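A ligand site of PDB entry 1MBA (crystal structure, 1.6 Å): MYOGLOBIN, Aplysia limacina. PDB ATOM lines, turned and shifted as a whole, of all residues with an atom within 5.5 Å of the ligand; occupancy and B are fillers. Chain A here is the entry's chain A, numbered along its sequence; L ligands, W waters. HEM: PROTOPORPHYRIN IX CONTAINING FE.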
ATOM      1  N   PHE A  29       6.533 -24.170 -10.661  1.00  0.00           N
ATOM      2  CA  PHE A  29       6.195 -22.828 -11.029  1.00  0.00           C
ATOM      3  C   PHE A  29       5.489 -22.803 -12.395  1.00  0.00           C
ATOM      4  O   PHE A  29       4.491 -22.145 -12.583  1.00  0.00           O
ATOM      5  CB  PHE A  29       7.476 -21.933 -11.041  1.00  0.00           C
ATOM      6  CG  PHE A  29       7.258 -20.628 -11.785  1.00  0.00           C
ATOM      7  CD1 PHE A  29       6.416 -19.637 -11.200  1.00  0.00           C
ATOM      8  CD2 PHE A  29       7.830 -20.384 -12.990  1.00  0.00           C
ATOM      9  CE1 PHE A  29       6.162 -18.430 -11.828  1.00  0.00           C
ATOM     10  CE2 PHE A  29       7.565 -19.127 -13.659  1.00  0.00           C
ATOM     11  CZ  PHE A  29       6.759 -18.186 -13.078  1.00  0.00           C
ATOM     12  N   LEU A  33       1.560 -21.850 -13.232  1.00  0.00           N
ATOM     13  CA  LEU A  33       1.283 -20.807 -14.203  1.00  0.00           C
ATOM     14  C   LEU A  33       0.258 -21.297 -15.184  1.00  0.00           C
ATOM     15  O   LEU A  33      -0.703 -20.606 -15.486  1.00  0.00           O
ATOM     16  CB  LEU A  33       2.557 -20.314 -14.973  1.00  0.00           C
ATOM     17  CG  LEU A  33       2.346 -19.175 -16.004  1.00  0.00           C
ATOM     18  CD1 LEU A  33       2.047 -17.844 -15.292  1.00  0.00           C
ATOM     19  CD2 LEU A  33       3.597 -19.050 -16.845  1.00  0.00           C
ATOM     20  N   SER A  40      -1.449 -19.234 -21.297  1.00  0.00           N
ATOM     21  CA  SER A  40       0.008 -19.145 -21.351  1.00  0.00           C
ATOM     22  C   SER A  40       0.681 -20.335 -22.023  1.00  0.00           C
ATOM     23  O   SER A  40       1.740 -20.183 -22.592  1.00  0.00           O
ATOM     24  CB  SER A  40       0.639 -18.788 -20.028  1.00  0.00           C
ATOM     25  OG  SER A  40       0.288 -19.776 -19.138  1.00  0.00           O
ATOM     26  N   PHE A  43       1.667 -20.340 -25.912  1.00  0.00           N
ATOM     27  CA  PHE A  43       2.843 -19.664 -26.491  1.00  0.00           C
ATOM     28  C   PHE A  43       3.987 -20.590 -26.674  1.00  0.00           C
ATOM     29  O   PHE A  43       4.902 -20.335 -27.458  1.00  0.00           O
ATOM     30  CB  PHE A  43       3.346 -18.521 -25.602  1.00  0.00           C
ATOM     31  CG  PHE A  43       2.351 -17.418 -25.544  1.00  0.00           C
ATOM     32  CD1 PHE A  43       2.355 -16.416 -26.539  1.00  0.00           C
ATOM     33  CD2 PHE A  43       1.434 -17.357 -24.547  1.00  0.00           C
ATOM     34  CE1 PHE A  43       1.432 -15.397 -26.487  1.00  0.00           C
ATOM     35  CE2 PHE A  43       0.478 -16.326 -24.485  1.00  0.00           C
ATOM     36  CZ  PHE A  43       0.496 -15.357 -25.455  1.00  0.00           C
ATOM     37  N   PHE A  44       3.951 -21.700 -25.924  1.00  0.00           N
ATOM     38  CA  PHE A  44       5.016 -22.701 -25.999  1.00  0.00           C
ATOM     39  C   PHE A  44       4.823 -23.743 -27.074  1.00  0.00           C
ATOM     40  O   PHE A  44       3.825 -24.455 -27.094  1.00  0.00           O
ATOM     41  CB  PHE A  44       5.170 -23.424 -24.628  1.00  0.00           C
ATOM     42  CG  PHE A  44       5.738 -22.570 -23.527  1.00  0.00           C
ATOM     43  CD1 PHE A  44       7.091 -22.542 -23.303  1.00  0.00           C
ATOM     44  CD2 PHE A  44       4.903 -21.799 -22.743  1.00  0.00           C
ATOM     45  CE1 PHE A  44       7.619 -21.739 -22.275  1.00  0.00           C
ATOM     46  CE2 PHE A  44       5.411 -20.988 -21.722  1.00  0.00           C
ATOM     47  CZ  PHE A  44       6.789 -20.975 -21.497  1.00  0.00           C
ATOM     48  N   ALA A  45       5.786 -23.834 -27.976  1.00  0.00           N
ATOM     49  CA  ALA A  45       5.733 -24.808 -29.077  1.00  0.00           C
ATOM     50  C   ALA A  45       5.564 -26.223 -28.552  1.00  0.00           C
ATOM     51  O   ALA A  45       4.806 -27.034 -29.100  1.00  0.00           O
ATOM     52  CB  ALA A  45       7.048 -24.794 -29.860  1.00  0.00           C
ATOM     53  N   ASP A  46       6.268 -26.513 -27.479  1.00  0.00           N
ATOM     54  CA  ASP A  46       6.249 -27.816 -26.860  1.00  0.00           C
ATOM     55  C   ASP A  46       5.011 -28.183 -26.076  1.00  0.00           C
ATOM     56  O   ASP A  46       4.746 -29.376 -25.924  1.00  0.00           O
ATOM     57  CB  ASP A  46       7.475 -28.050 -25.934  1.00  0.00           C
ATOM     58  CG  ASP A  46       8.880 -27.831 -26.537  1.00  0.00           C
ATOM     59  OD1 ASP A  46       9.647 -27.061 -26.084  1.00  0.00           O
ATOM     60  OD2 ASP A  46       9.175 -28.569 -27.567  1.00  0.00           O
ATOM     61  N   VAL A  64      12.585 -26.693 -20.158  1.00  0.00           N
ATOM     62  CA  VAL A  64      11.984 -25.374 -20.162  1.00  0.00           C
ATOM     63  C   VAL A  64      11.965 -24.698 -18.784  1.00  0.00           C
ATOM     64  O   VAL A  64      12.347 -23.542 -18.647  1.00  0.00           O
ATOM     65  CB  VAL A  64      10.511 -25.413 -20.743  1.00  0.00           C
ATOM     66  CG1 VAL A  64       9.838 -24.022 -20.867  1.00  0.00           C
ATOM     67  CG2 VAL A  64      10.457 -26.183 -22.069  1.00  0.00           C
ATOM     68  N   ARG A  67      15.584 -23.586 -17.552  1.00  0.00           N
ATOM     69  CA  ARG A  67      16.094 -22.372 -18.217  1.00  0.00           C
ATOM     70  C   ARG A  67      15.455 -21.113 -17.617  1.00  0.00           C
ATOM     71  O   ARG A  67      16.086 -20.090 -17.424  1.00  0.00           O
ATOM     72  CB  ARG A  67      15.979 -22.450 -19.732  1.00  0.00           C
ATOM     73  CG  ARG A  67      17.014 -23.381 -20.298  1.00  0.00           C
ATOM     74  CD  ARG A  67      16.769 -23.769 -21.750  1.00  0.00           C
ATOM     75  NE  ARG A  67      17.885 -24.550 -22.277  1.00  0.00           N
ATOM     76  CZ  ARG A  67      18.202 -24.595 -23.546  1.00  0.00           C
ATOM     77  NH1 ARG A  67      17.512 -23.924 -24.459  1.00  0.00           N
ATOM     78  NH2 ARG A  67      19.241 -25.340 -23.945  1.00  0.00           N
ATOM     79  N   ILE A  68      14.159 -21.207 -17.288  1.00  0.00           N
ATOM     80  CA  ILE A  68      13.454 -20.085 -16.683  1.00  0.00           C
ATOM     81  C   ILE A  68      14.033 -19.758 -15.306  1.00  0.00           C
ATOM     82  O   ILE A  68      14.327 -18.609 -14.992  1.00  0.00           O
ATOM     83  CB  ILE A  68      11.951 -20.374 -16.550  1.00  0.00           C
ATOM     84  CG1 ILE A  68      11.263 -20.319 -17.885  1.00  0.00           C
ATOM     85  CG2 ILE A  68      11.220 -19.443 -15.533  1.00  0.00           C
ATOM     86  CD1 ILE A  68       9.886 -20.988 -17.844  1.00  0.00           C
ATOM     87  N   ARG A  71      17.533 -18.166 -15.407  1.00  0.00           N
ATOM     88  CA  ARG A  71      17.486 -16.766 -15.746  1.00  0.00           C
ATOM     89  C   ARG A  71      16.926 -15.878 -14.612  1.00  0.00           C
ATOM     90  O   ARG A  71      17.452 -14.798 -14.332  1.00  0.00           O
ATOM     91  CB  ARG A  71      16.797 -16.534 -17.110  1.00  0.00           C
ATOM     92  CG  ARG A  71      16.754 -15.071 -17.567  1.00  0.00           C
ATOM     93  CD  ARG A  71      18.103 -14.549 -18.095  1.00  0.00           C
ATOM     94  NE  ARG A  71      18.501 -15.429 -19.180  1.00  0.00           N
ATOM     95  CZ  ARG A  71      18.196 -15.148 -20.472  1.00  0.00           C
ATOM     96  NH1 ARG A  71      17.521 -14.050 -20.816  1.00  0.00           N
ATOM     97  NH2 ARG A  71      18.563 -15.984 -21.434  1.00  0.00           N
ATOM     98  N   LEU A  72      15.868 -16.358 -13.934  1.00  0.00           N
ATOM     99  CA  LEU A  72      15.266 -15.623 -12.826  1.00  0.00           C
ATOM    100  C   LEU A  72      16.260 -15.389 -11.685  1.00  0.00           C
ATOM    101  O   LEU A  72      16.258 -14.346 -11.032  1.00  0.00           O
ATOM    102  CB  LEU A  72      14.086 -16.401 -12.199  1.00  0.00           C
ATOM    103  CG  LEU A  72      12.751 -15.670 -12.123  1.00  0.00           C
ATOM    104  CD1 LEU A  72      11.734 -16.395 -11.229  1.00  0.00           C
ATOM    105  CD2 LEU A  72      12.817 -14.145 -11.939  1.00  0.00           C
ATOM    106  N   PHE A  75      18.308 -12.553 -12.606  1.00  0.00           N
ATOM    107  CA  PHE A  75      17.618 -11.285 -12.394  1.00  0.00           C
ATOM    108  C   PHE A  75      17.711 -10.889 -10.933  1.00  0.00           C
ATOM    109  O   PHE A  75      17.963  -9.754 -10.620  1.00  0.00           O
ATOM    110  CB  PHE A  75      16.132 -11.302 -12.801  1.00  0.00           C
ATOM    111  CG  PHE A  75      15.897 -10.961 -14.240  1.00  0.00           C
ATOM    112  CD1 PHE A  75      15.385 -11.873 -15.091  1.00  0.00           C
ATOM    113  CD2 PHE A  75      16.183  -9.639 -14.733  1.00  0.00           C
ATOM    114  CE1 PHE A  75      15.153 -11.568 -16.448  1.00  0.00           C
ATOM    115  CE2 PHE A  75      15.961  -9.330 -16.023  1.00  0.00           C
ATOM    116  CZ  PHE A  75      15.433 -10.324 -16.901  1.00  0.00           C
ATOM    117  N   PHE A  92      16.096  -9.723 -22.558  1.00  0.00           N
ATOM    118  CA  PHE A  92      14.956 -10.504 -22.164  1.00  0.00           C
ATOM    119  C   PHE A  92      13.722 -10.188 -22.989  1.00  0.00           C
ATOM    120  O   PHE A  92      13.103 -11.056 -23.584  1.00  0.00           O
ATOM    121  CB  PHE A  92      14.591 -10.266 -20.726  1.00  0.00           C
ATOM    122  CG  PHE A  92      13.602 -11.234 -20.170  1.00  0.00           C
ATOM    123  CD1 PHE A  92      13.994 -12.514 -19.840  1.00  0.00           C
ATOM    124  CD2 PHE A  92      12.275 -10.860 -19.982  1.00  0.00           C
ATOM    125  CE1 PHE A  92      13.092 -13.421 -19.312  1.00  0.00           C
ATOM    126  CE2 PHE A  92      11.341 -11.751 -19.461  1.00  0.00           C
ATOM    127  CZ  PHE A  92      11.770 -13.038 -19.128  1.00  0.00           C
ATOM    128  N   GLU A  95      13.972 -11.073 -26.769  1.00  0.00           N
ATOM    129  CA  GLU A  95      13.740 -12.474 -26.955  1.00  0.00           C
ATOM    130  C   GLU A  95      12.255 -12.871 -26.861  1.00  0.00           C
ATOM    131  O   GLU A  95      11.723 -13.541 -27.738  1.00  0.00           O
ATOM    132  CB  GLU A  95      14.484 -13.273 -25.881  1.00  0.00           C
ATOM    133  CG  GLU A  95      16.010 -13.138 -25.914  1.00  0.00           C
ATOM    134  CD  GLU A  95      16.666 -14.334 -25.288  1.00  0.00           C
ATOM    135  OE1 GLU A  95      16.096 -15.391 -25.204  1.00  0.00           O
ATOM    136  OE2 GLU A  95      17.867 -14.133 -24.809  1.00  0.00           O
ATOM    137  N   HIS A  96      11.580 -12.436 -25.799  1.00  0.00           N
ATOM    138  CA  HIS A  96      10.151 -12.737 -25.554  1.00  0.00           C
ATOM    139  C   HIS A  96       9.176 -12.267 -26.620  1.00  0.00           C
ATOM    140  O   HIS A  96       8.262 -12.992 -26.987  1.00  0.00           O
ATOM    141  CB  HIS A  96       9.683 -12.463 -24.068  1.00  0.00           C
ATOM    142  CG  HIS A  96      10.250 -13.614 -23.237  1.00  0.00           C
ATOM    143  ND1 HIS A  96      11.556 -13.623 -22.794  1.00  0.00           N
ATOM    144  CD2 HIS A  96       9.656 -14.764 -22.818  1.00  0.00           C
ATOM    145  CE1 HIS A  96      11.719 -14.746 -22.108  1.00  0.00           C
ATOM    146  NE2 HIS A  96      10.616 -15.455 -22.098  1.00  0.00           N
ATOM    147  N   PHE A  99       8.857 -14.311 -29.674  1.00  0.00           N
ATOM    148  CA  PHE A  99       8.066 -15.487 -29.509  1.00  0.00           C
ATOM    149  C   PHE A  99       6.595 -15.147 -29.407  1.00  0.00           C
ATOM    150  O   PHE A  99       5.764 -16.021 -29.326  1.00  0.00           O
ATOM    151  CB  PHE A  99       8.477 -16.291 -28.266  1.00  0.00           C
ATOM    152  CG  PHE A  99       9.911 -16.816 -28.250  1.00  0.00           C
ATOM    153  CD1 PHE A  99      10.400 -17.641 -29.245  1.00  0.00           C
ATOM    154  CD2 PHE A  99      10.772 -16.503 -27.187  1.00  0.00           C
ATOM    155  CE1 PHE A  99      11.709 -18.112 -29.198  1.00  0.00           C
ATOM    156  CE2 PHE A  99      12.091 -16.971 -27.121  1.00  0.00           C
ATOM    157  CZ  PHE A  99      12.551 -17.777 -28.139  1.00  0.00           C
ATOM    158  N   VAL A 101       5.239 -13.202 -26.942  1.00  0.00           N
ATOM    159  CA  VAL A 101       4.925 -12.975 -25.565  1.00  0.00           C
ATOM    160  C   VAL A 101       5.029 -11.470 -25.228  1.00  0.00           C
ATOM    161  O   VAL A 101       6.010 -10.801 -25.582  1.00  0.00           O
ATOM    162  CB  VAL A 101       5.809 -13.873 -24.641  1.00  0.00           C
ATOM    163  CG1 VAL A 101       5.287 -13.839 -23.212  1.00  0.00           C
ATOM    164  CG2 VAL A 101       5.956 -15.318 -25.135  1.00  0.00           C
ATOM    165  N   GLN A 105       1.266 -11.150 -20.344  1.00  0.00           N
ATOM    166  CA  GLN A 105       1.642 -12.457 -19.813  1.00  0.00           C
ATOM    167  C   GLN A 105       2.456 -12.329 -18.545  1.00  0.00           C
ATOM    168  O   GLN A 105       2.392 -13.185 -17.685  1.00  0.00           O
ATOM    169  CB  GLN A 105       2.416 -13.343 -20.795  1.00  0.00           C
ATOM    170  CG  GLN A 105       1.562 -13.987 -21.895  1.00  0.00           C
ATOM    171  CD  GLN A 105       0.884 -13.034 -22.818  1.00  0.00           C
ATOM    172  OE1 GLN A 105      -0.332 -13.095 -22.945  1.00  0.00           O
ATOM    173  NE2 GLN A 105       1.617 -12.136 -23.412  1.00  0.00           N
ATOM    174  N   PHE A 106       3.237 -11.237 -18.466  1.00  0.00           N
ATOM    175  CA  PHE A 106       4.073 -10.937 -17.331  1.00  0.00           C
ATOM    176  C   PHE A 106       3.244 -10.401 -16.180  1.00  0.00           C
ATOM    177  O   PHE A 106       3.586 -10.580 -15.020  1.00  0.00           O
ATOM    178  CB  PHE A 106       5.353 -10.156 -17.687  1.00  0.00           C
ATOM    179  CG  PHE A 106       6.338 -11.170 -18.226  1.00  0.00           C
ATOM    180  CD1 PHE A 106       7.237 -11.783 -17.375  1.00  0.00           C
ATOM    181  CD2 PHE A 106       6.361 -11.539 -19.599  1.00  0.00           C
ATOM    182  CE1 PHE A 106       8.156 -12.741 -17.859  1.00  0.00           C
ATOM    183  CE2 PHE A 106       7.252 -12.474 -20.093  1.00  0.00           C
ATOM    184  CZ  PHE A 106       8.170 -13.082 -19.187  1.00  0.00           C
ATOM    185  N   VAL A 109       2.203 -13.369 -14.539  1.00  0.00           N
ATOM    186  CA  VAL A 109       3.271 -13.934 -13.721  1.00  0.00           C
ATOM    187  C   VAL A 109       3.362 -13.172 -12.393  1.00  0.00           C
ATOM    188  O   VAL A 109       3.434 -13.771 -11.321  1.00  0.00           O
ATOM    189  CB  VAL A 109       4.634 -13.937 -14.407  1.00  0.00           C
ATOM    190  CG1 VAL A 109       5.666 -14.381 -13.372  1.00  0.00           C
ATOM    191  CG2 VAL A 109       4.600 -14.906 -15.623  1.00  0.00           C
ATOM    192  N   PHE A 135       9.112  -7.434 -11.346  1.00  0.00           N
ATOM    193  CA  PHE A 135       8.274  -7.861 -12.455  1.00  0.00           C
ATOM    194  C   PHE A 135       7.840  -6.640 -13.242  1.00  0.00           C
ATOM    195  O   PHE A 135       7.673  -6.691 -14.446  1.00  0.00           O
ATOM    196  CB  PHE A 135       7.111  -8.789 -12.000  1.00  0.00           C
ATOM    197  CG  PHE A 135       7.616 -10.213 -11.840  1.00  0.00           C
ATOM    198  CD1 PHE A 135       7.539 -10.841 -10.677  1.00  0.00           C
ATOM    199  CD2 PHE A 135       8.206 -10.844 -12.963  1.00  0.00           C
ATOM    200  CE1 PHE A 135       8.049 -12.200 -10.560  1.00  0.00           C
ATOM    201  CE2 PHE A 135       8.684 -12.120 -12.869  1.00  0.00           C
ATOM    202  CZ  PHE A 135       8.593 -12.798 -11.622  1.00  0.00           C
HETATM  203  CHA HEM L   1      12.102 -18.961 -23.701  1.00  0.00           C
HETATM  204  CHB HEM L   1      13.008 -17.070 -19.275  1.00  0.00           C
HETATM  205  CHC HEM L   1       8.287 -16.299 -18.625  1.00  0.00           C
HETATM  206  CHD HEM L   1       7.443 -18.005 -23.043  1.00  0.00           C
HETATM  207  C1A HEM L   1      12.761 -18.558 -22.527  1.00  0.00           C
HETATM  208  C2A HEM L   1      14.226 -18.535 -22.356  1.00  0.00           C
HETATM  209  C3A HEM L   1      14.451 -18.017 -21.119  1.00  0.00           C
HETATM  210  C4A HEM L   1      13.175 -17.665 -20.547  1.00  0.00           C
HETATM  211  CMA HEM L   1      15.793 -17.798 -20.369  1.00  0.00           C
HETATM  212  CAA HEM L   1      15.225 -19.062 -23.441  1.00  0.00           C
HETATM  213  CBA HEM L   1      15.580 -20.542 -23.195  1.00  0.00           C
HETATM  214  CGA HEM L   1      16.626 -21.101 -24.139  1.00  0.00           C
HETATM  215  O1A HEM L   1      17.813 -21.142 -23.749  1.00  0.00           O
HETATM  216  O2A HEM L   1      16.298 -21.433 -25.284  1.00  0.00           O
HETATM  217  C1B HEM L   1      11.807 -16.690 -18.707  1.00  0.00           C
HETATM  218  C2B HEM L   1      11.655 -16.126 -17.380  1.00  0.00           C
HETATM  219  C3B HEM L   1      10.342 -16.029 -17.120  1.00  0.00           C
HETATM  220  C4B HEM L   1       9.656 -16.354 -18.419  1.00  0.00           C
HETATM  221  CMB HEM L   1      12.831 -15.742 -16.454  1.00  0.00           C
HETATM  222  CAB HEM L   1       9.696 -15.353 -15.878  1.00  0.00           C
HETATM  223  CBB HEM L   1       8.994 -15.951 -14.941  1.00  0.00           C
HETATM  224  C1C HEM L   1       7.648 -16.655 -19.784  1.00  0.00           C
HETATM  225  C2C HEM L   1       6.177 -16.633 -20.001  1.00  0.00           C
HETATM  226  C3C HEM L   1       6.013 -17.175 -21.234  1.00  0.00           C
HETATM  227  C4C HEM L   1       7.302 -17.503 -21.772  1.00  0.00           C
HETATM  228  CMC HEM L   1       5.121 -16.133 -19.009  1.00  0.00           C
HETATM  229  CAC HEM L   1       4.715 -17.415 -22.025  1.00  0.00           C
HETATM  230  CBC HEM L   1       3.581 -17.076 -21.434  1.00  0.00           C
HETATM  231  C1D HEM L   1       8.623 -18.379 -23.647  1.00  0.00           C
HETATM  232  C2D HEM L   1       8.740 -18.975 -24.955  1.00  0.00           C
HETATM  233  C3D HEM L   1      10.034 -19.267 -25.120  1.00  0.00           C
HETATM  234  C4D HEM L   1      10.739 -18.800 -23.942  1.00  0.00           C
HETATM  235  CMD HEM L   1       7.570 -19.348 -25.901  1.00  0.00           C
HETATM  236  CAD HEM L   1      10.686 -19.973 -26.313  1.00  0.00           C
HETATM  237  CBD HEM L   1      11.533 -21.210 -25.962  1.00  0.00           C
HETATM  238  CGD HEM L   1      10.689 -22.382 -26.321  1.00  0.00           C
HETATM  239  O1D HEM L   1       9.525 -22.339 -25.919  1.00  0.00           O
HETATM  240  O2D HEM L   1      11.169 -23.370 -26.903  1.00  0.00           O
HETATM  241  NA  HEM L   1      12.158 -18.002 -21.419  1.00  0.00           N
HETATM  242  NB  HEM L   1      10.584 -16.725 -19.361  1.00  0.00           N
HETATM  243  NC  HEM L   1       8.307 -17.185 -20.875  1.00  0.00           N
HETATM  244  ND  HEM L   1       9.853 -18.237 -23.075  1.00  0.00           N
HETATM  245 FE   HEM L   1      10.246 -17.352 -21.258  1.00  0.00          FE
HETATM  246  O   HOH W   1       8.189 -24.685 -26.229  1.00  0.00           O
HETATM  247  O   HOH W   2      12.161 -21.562 -21.157  1.00  0.00           O
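Water W1 lies within hydrogen-bond range of an oxygen (O1D) of the ligand (2.7 Å), the side-chain carboxylate of Asp 46 (2.8 Å) and the backbone NH of Ala 45 (3.1 Å).
Phe 29 touches the ligand.
Leu 33 touches the ligand.
Ser 40 touches the ligand (CB to CBC, 3.7 Å).
O of Phe 43 touches CMD of the ligand (3.2 Å).
Phe 44 touches the ligand (CZ to CHD, 3.4 Å).
O of Ile 68 touches CMB of the ligand, at 3.5 Å.
Arg 71 touches the ligand.
N of Leu 72 touches CMB of the ligand (3.99 Å).
Phe 92 touches the ligand.
Phe 99 touches the ligand (CZ to CAD, 3.4 Å).
CG2 of Val 101 touches CHD of the ligand, at 3.7 Å.
Gln 105 touches the ligand (CG to CBC, 3.7 Å).
Phe 106 touches the ligand (CZ to CHC, 3.3 Å).
Val 109 touches the ligand (CG2 to CMC, 3.6 Å).
Hydrophobic or aromatic side chains that line the ligand: Phe 29, Leu 33, Phe 43, Phe 44, Ile 68, Phe 92, His 96, Phe 99, Val 101, Phe 106 and Val 109.
16 residues have an atom within 4 Å of the ligand: Phe 29, Leu 33, Ser 40, Phe 43, Phe 44, Arg 67, Ile 68, Arg 71, Leu 72, Phe 92, His 96, Phe 99, Val 101, Gln 105, Phe 106 and Val 109.
The nearest printed residue that does not touch the ligand is Asp 46 (4.1 Å).
An iron atom (FE) of the ligand is bound by a ring nitrogen (NE2) of His 96 (2.1 Å).
An oxygen (O1A) of the ligand is in salt-bridge range of the guanidinium group (NH1) of Arg 67, 2.9 Å away.
The backbone carbonyl oxygen (O) of His 96 lies within hydrogen-bond range of the backbone NH (N) of Val 101.
The guanidinium group (NH2) of Arg 71 lies within salt-bridge range of the side-chain carboxylate (OE2) of Glu 95 (3.9 Å).
A ring nitrogen (ND1) of His 96 is in hydrogen-bond range of the backbone carbonyl oxygen of Phe 92, 3.1 Å away.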
